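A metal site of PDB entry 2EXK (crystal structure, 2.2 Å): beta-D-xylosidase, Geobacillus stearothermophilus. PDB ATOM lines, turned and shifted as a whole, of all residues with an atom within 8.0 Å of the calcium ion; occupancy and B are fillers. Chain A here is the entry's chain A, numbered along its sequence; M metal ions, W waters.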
ATOM      1  N   LYS A 331      24.538 -31.721  -9.040  1.00  0.00           N
ATOM      2  CA  LYS A 331      24.026 -31.223  -7.784  1.00  0.00           C
ATOM      3  C   LYS A 331      22.839 -30.319  -8.081  1.00  0.00           C
ATOM      4  O   LYS A 331      23.008 -29.160  -8.458  1.00  0.00           O
ATOM      5  CB  LYS A 331      25.104 -30.473  -7.003  1.00  0.00           C
ATOM      6  CG  LYS A 331      24.665 -30.043  -5.601  1.00  0.00           C
ATOM      7  CD  LYS A 331      25.753 -29.244  -4.913  1.00  0.00           C
ATOM      8  CE  LYS A 331      25.327 -28.838  -3.520  1.00  0.00           C
ATOM      9  NZ  LYS A 331      26.377 -28.070  -2.781  1.00  0.00           N
ATOM     10  N   ASP A 332      21.652 -30.874  -7.897  1.00  0.00           N
ATOM     11  CA  ASP A 332      20.394 -30.204  -8.205  1.00  0.00           C
ATOM     12  C   ASP A 332      19.997 -29.378  -6.993  1.00  0.00           C
ATOM     13  O   ASP A 332      19.570 -29.917  -5.977  1.00  0.00           O
ATOM     14  CB  ASP A 332      19.306 -31.232  -8.535  1.00  0.00           C
ATOM     15  CG  ASP A 332      17.963 -30.589  -8.930  1.00  0.00           C
ATOM     16  OD1 ASP A 332      17.738 -29.386  -8.627  1.00  0.00           O
ATOM     17  OD2 ASP A 332      17.128 -31.299  -9.534  1.00  0.00           O
ATOM     18  N   ASP A 333      20.161 -28.067  -7.114  1.00  0.00           N
ATOM     19  CA  ASP A 333      19.877 -27.147  -6.024  1.00  0.00           C
ATOM     20  C   ASP A 333      18.400 -26.781  -5.828  1.00  0.00           C
ATOM     21  O   ASP A 333      18.099 -25.954  -4.973  1.00  0.00           O
ATOM     22  CB  ASP A 333      20.684 -25.865  -6.202  1.00  0.00           C
ATOM     23  CG  ASP A 333      21.764 -25.725  -5.163  1.00  0.00           C
ATOM     24  OD1 ASP A 333      21.444 -25.765  -3.929  1.00  0.00           O
ATOM     25  OD2 ASP A 333      22.927 -25.554  -5.579  1.00  0.00           O
ATOM     26  N   PHE A 334      17.511 -27.402  -6.608  1.00  0.00           N
ATOM     27  CA  PHE A 334      16.068 -27.095  -6.540  1.00  0.00           C
ATOM     28  C   PHE A 334      15.824 -25.612  -6.841  1.00  0.00           C
ATOM     29  O   PHE A 334      15.211 -24.866  -6.056  1.00  0.00           O
ATOM     30  CB  PHE A 334      15.450 -27.549  -5.210  1.00  0.00           C
ATOM     31  CG  PHE A 334      15.569 -29.041  -4.962  1.00  0.00           C
ATOM     32  CD1 PHE A 334      15.121 -29.953  -5.910  1.00  0.00           C
ATOM     33  CD2 PHE A 334      16.136 -29.529  -3.793  1.00  0.00           C
ATOM     34  CE1 PHE A 334      15.243 -31.331  -5.693  1.00  0.00           C
ATOM     35  CE2 PHE A 334      16.251 -30.907  -3.565  1.00  0.00           C
ATOM     36  CZ  PHE A 334      15.803 -31.807  -4.520  1.00  0.00           C
ATOM     37  N   ASP A 335      16.331 -25.209  -8.007  1.00  0.00           N
ATOM     38  CA  ASP A 335      16.320 -23.817  -8.463  1.00  0.00           C
ATOM     39  C   ASP A 335      15.117 -23.512  -9.362  1.00  0.00           C
ATOM     40  O   ASP A 335      14.661 -22.367  -9.412  1.00  0.00           O
ATOM     41  CB  ASP A 335      17.602 -23.490  -9.238  1.00  0.00           C
ATOM     42  CG  ASP A 335      18.824 -23.420  -8.351  1.00  0.00           C
ATOM     43  OD1 ASP A 335      18.721 -22.934  -7.198  1.00  0.00           O
ATOM     44  OD2 ASP A 335      19.911 -23.828  -8.824  1.00  0.00           O
ATOM     45  N   LEU A 357       8.226 -26.433  -4.187  1.00  0.00           N
ATOM     46  CA  LEU A 357       9.399 -25.550  -4.264  1.00  0.00           C
ATOM     47  C   LEU A 357       9.073 -24.138  -3.765  1.00  0.00           C
ATOM     48  O   LEU A 357       9.955 -23.270  -3.706  1.00  0.00           O
ATOM     49  CB  LEU A 357       9.906 -25.444  -5.705  1.00  0.00           C
ATOM     50  CG  LEU A 357      10.768 -26.505  -6.386  1.00  0.00           C
ATOM     51  CD1 LEU A 357      11.768 -27.183  -5.438  1.00  0.00           C
ATOM     52  CD2 LEU A 357       9.926 -27.529  -7.079  1.00  0.00           C
ATOM     53  N   ARG A 360       9.832 -22.870   0.726  1.00  0.00           N
ATOM     54  CA  ARG A 360      11.143 -22.368   1.127  1.00  0.00           C
ATOM     55  C   ARG A 360      11.999 -22.269  -0.097  1.00  0.00           C
ATOM     56  O   ARG A 360      12.337 -23.284  -0.696  1.00  0.00           O
ATOM     57  CB  ARG A 360      11.827 -23.289   2.161  1.00  0.00           C
ATOM     58  CG  ARG A 360      12.993 -22.606   2.906  1.00  0.00           C
ATOM     59  CD  ARG A 360      13.864 -23.617   3.656  1.00  0.00           C
ATOM     60  NE  ARG A 360      14.998 -22.997   4.346  1.00  0.00           N
ATOM     61  CZ  ARG A 360      15.655 -23.548   5.364  1.00  0.00           C
ATOM     62  NH1 ARG A 360      15.300 -24.741   5.841  1.00  0.00           N
ATOM     63  NH2 ARG A 360      16.671 -22.913   5.923  1.00  0.00           N
ATOM     64  N   PRO A 361      12.391 -21.033  -0.484  1.00  0.00           N
ATOM     65  CA  PRO A 361      13.128 -20.832  -1.741  1.00  0.00           C
ATOM     66  C   PRO A 361      14.357 -21.740  -1.834  1.00  0.00           C
ATOM     67  O   PRO A 361      15.094 -21.911  -0.850  1.00  0.00           O
ATOM     68  CB  PRO A 361      13.530 -19.349  -1.689  1.00  0.00           C
ATOM     69  CG  PRO A 361      12.529 -18.708  -0.796  1.00  0.00           C
ATOM     70  CD  PRO A 361      12.182 -19.765   0.237  1.00  0.00           C
ATOM     71  N   GLY A 362      14.543 -22.325  -3.011  1.00  0.00           N
ATOM     72  CA  GLY A 362      15.696 -23.178  -3.285  1.00  0.00           C
ATOM     73  C   GLY A 362      15.709 -24.487  -2.520  1.00  0.00           C
ATOM     74  O   GLY A 362      16.756 -25.103  -2.368  1.00  0.00           O
ATOM     75  N   HIS A 363      14.545 -24.909  -2.038  1.00  0.00           N
ATOM     76  CA  HIS A 363      14.436 -26.173  -1.332  1.00  0.00           C
ATOM     77  C   HIS A 363      13.245 -26.915  -1.868  1.00  0.00           C
ATOM     78  O   HIS A 363      12.243 -26.296  -2.250  1.00  0.00           O
ATOM     79  CB  HIS A 363      14.202 -25.944   0.164  1.00  0.00           C
ATOM     80  CG  HIS A 363      15.394 -25.417   0.891  1.00  0.00           C
ATOM     81  ND1 HIS A 363      15.895 -24.145   0.705  1.00  0.00           N
ATOM     82  CD2 HIS A 363      16.153 -25.984   1.863  1.00  0.00           C
ATOM     83  CE1 HIS A 363      16.936 -23.968   1.487  1.00  0.00           C
ATOM     84  NE2 HIS A 363      17.107 -25.063   2.209  1.00  0.00           N
ATOM     85  N   LEU A 364      13.337 -28.240  -1.895  1.00  0.00           N
ATOM     86  CA  LEU A 364      12.155 -29.060  -2.041  1.00  0.00           C
ATOM     87  C   LEU A 364      11.615 -29.307  -0.645  1.00  0.00           C
ATOM     88  O   LEU A 364      12.301 -29.834   0.215  1.00  0.00           O
ATOM     89  CB  LEU A 364      12.444 -30.388  -2.763  1.00  0.00           C
ATOM     90  CG  LEU A 364      11.304 -31.432  -2.791  1.00  0.00           C
ATOM     91  CD1 LEU A 364      10.111 -30.960  -3.676  1.00  0.00           C
ATOM     92  CD2 LEU A 364      11.802 -32.776  -3.282  1.00  0.00           C
ATOM     93  N   LYS A 395      20.721 -32.860   1.495  1.00  0.00           N
ATOM     94  CA  LYS A 395      21.023 -31.990   2.617  1.00  0.00           C
ATOM     95  C   LYS A 395      19.667 -31.523   3.148  1.00  0.00           C
ATOM     96  O   LYS A 395      18.935 -30.850   2.433  1.00  0.00           O
ATOM     97  CB  LYS A 395      21.877 -30.803   2.160  1.00  0.00           C
ATOM     98  CG  LYS A 395      22.097 -29.691   3.198  1.00  0.00           C
ATOM     99  CD  LYS A 395      22.688 -28.445   2.543  1.00  0.00           C
ATOM    100  CE  LYS A 395      22.656 -27.255   3.483  1.00  0.00           C
ATOM    101  NZ  LYS A 395      23.101 -25.968   2.878  1.00  0.00           N
ATOM    102  N   TYR A 460      21.102 -28.498   9.304  1.00  0.00           N
ATOM    103  CA  TYR A 460      21.064 -29.429   8.187  1.00  0.00           C
ATOM    104  C   TYR A 460      21.843 -30.681   8.505  1.00  0.00           C
ATOM    105  O   TYR A 460      22.946 -30.610   9.034  1.00  0.00           O
ATOM    106  CB  TYR A 460      21.679 -28.810   6.947  1.00  0.00           C
ATOM    107  CG  TYR A 460      20.847 -27.744   6.279  1.00  0.00           C
ATOM    108  CD1 TYR A 460      19.740 -28.084   5.505  1.00  0.00           C
ATOM    109  CD2 TYR A 460      21.178 -26.396   6.412  1.00  0.00           C
ATOM    110  CE1 TYR A 460      18.975 -27.114   4.871  1.00  0.00           C
ATOM    111  CE2 TYR A 460      20.437 -25.410   5.768  1.00  0.00           C
ATOM    112  CZ  TYR A 460      19.334 -25.774   4.996  1.00  0.00           C
ATOM    113  OH  TYR A 460      18.588 -24.809   4.358  1.00  0.00           O
ATOM    114  N   PHE A 527      14.629 -29.979   1.792  1.00  0.00           N
ATOM    115  CA  PHE A 527      15.801 -30.547   1.130  1.00  0.00           C
ATOM    116  C   PHE A 527      16.501 -29.476   0.309  1.00  0.00           C
ATOM    117  O   PHE A 527      15.950 -29.004  -0.667  1.00  0.00           O
ATOM    118  CB  PHE A 527      15.394 -31.734   0.233  1.00  0.00           C
ATOM    119  CG  PHE A 527      14.814 -32.901   1.004  1.00  0.00           C
ATOM    120  CD1 PHE A 527      15.636 -33.952   1.423  1.00  0.00           C
ATOM    121  CD2 PHE A 527      13.467 -32.924   1.339  1.00  0.00           C
ATOM    122  CE1 PHE A 527      15.108 -35.021   2.159  1.00  0.00           C
ATOM    123  CE2 PHE A 527      12.939 -33.994   2.075  1.00  0.00           C
ATOM    124  CZ  PHE A 527      13.775 -35.027   2.486  1.00  0.00           C
ATOM    125  N   ASP A 528      17.715 -29.111   0.700  1.00  0.00           N
ATOM    126  CA  ASP A 528      18.429 -28.023   0.030  1.00  0.00           C
ATOM    127  C   ASP A 528      18.879 -28.402  -1.381  1.00  0.00           C
ATOM    128  O   ASP A 528      18.816 -27.573  -2.295  1.00  0.00           O
ATOM    129  CB  ASP A 528      19.618 -27.561   0.855  1.00  0.00           C
ATOM    130  CG  ASP A 528      20.241 -26.275   0.312  1.00  0.00           C
ATOM    131  OD1 ASP A 528      21.351 -25.953   0.721  1.00  0.00           O
ATOM    132  OD2 ASP A 528      19.610 -25.576  -0.531  1.00  0.00           O
ATOM    133  N   TYR A 529      19.332 -29.634  -1.567  1.00  0.00           N
ATOM    134  CA  TYR A 529      19.711 -30.113  -2.898  1.00  0.00           C
ATOM    135  C   TYR A 529      19.575 -31.619  -3.018  1.00  0.00           C
ATOM    136  O   TYR A 529      19.323 -32.311  -2.026  1.00  0.00           O
ATOM    137  CB  TYR A 529      21.136 -29.658  -3.251  1.00  0.00           C
ATOM    138  CG  TYR A 529      22.230 -30.215  -2.361  1.00  0.00           C
ATOM    139  CD1 TYR A 529      22.751 -31.488  -2.571  1.00  0.00           C
ATOM    140  CD2 TYR A 529      22.735 -29.465  -1.312  1.00  0.00           C
ATOM    141  CE1 TYR A 529      23.751 -32.009  -1.748  1.00  0.00           C
ATOM    142  CE2 TYR A 529      23.752 -29.970  -0.487  1.00  0.00           C
ATOM    143  CZ  TYR A 529      24.236 -31.235  -0.720  1.00  0.00           C
ATOM    144  OH  TYR A 529      25.232 -31.732   0.100  1.00  0.00           O
ATOM    145  N   PHE A 530      19.728 -32.144  -4.223  1.00  0.00           N
ATOM    146  CA  PHE A 530      19.828 -33.587  -4.413  1.00  0.00           C
ATOM    147  C   PHE A 530      20.880 -33.835  -5.457  1.00  0.00           C
ATOM    148  O   PHE A 530      20.720 -33.420  -6.597  1.00  0.00           O
ATOM    149  CB  PHE A 530      18.513 -34.249  -4.817  1.00  0.00           C
ATOM    150  CG  PHE A 530      18.596 -35.761  -4.917  1.00  0.00           C
ATOM    151  CD1 PHE A 530      18.383 -36.563  -3.784  1.00  0.00           C
ATOM    152  CD2 PHE A 530      18.895 -36.382  -6.114  1.00  0.00           C
ATOM    153  CE1 PHE A 530      18.457 -37.947  -3.856  1.00  0.00           C
ATOM    154  CE2 PHE A 530      18.970 -37.784  -6.203  1.00  0.00           C
ATOM    155  CZ  PHE A 530      18.740 -38.569  -5.072  1.00  0.00           C
HETATM  156 CA    CA M   1      18.956 -25.207  -2.796  1.00  0.00          CA
HETATM  157  O   HOH W   1      19.034 -23.059  -1.762  1.00  0.00           O
HETATM  158  O   HOH W   2      19.073 -23.301  -4.663  1.00  0.00           O
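The side-chain amino group (NZ) of Lys 395 lies within salt-bridge range of the side-chain carboxylate (OD1) of Asp 528 (2.8 Å).
Of the 17 residues printed, 3 come within 4 Å of the calcium ion.
The nearest printed residue that does not touch the calcium ion is His 363 (4.5 Å).
The calcium ion is bound by the backbone carbonyl oxygen (O) of Gly 362 (2.2 Å), water W1 (2.4 Å), the side-chain carboxylate (OD2) of Asp 528 (2.4 Å), the backbone carbonyl oxygen (O) of Asp 528 (2.4 Å), the backbone carbonyl oxygen (O) of Asp 333 (2.5 Å), water W2 (2.7 Å) and the side-chain carboxylate (OD1) of Asp 333 (2.8 Å).
The calcium ion has seven donor atoms within binding distance.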
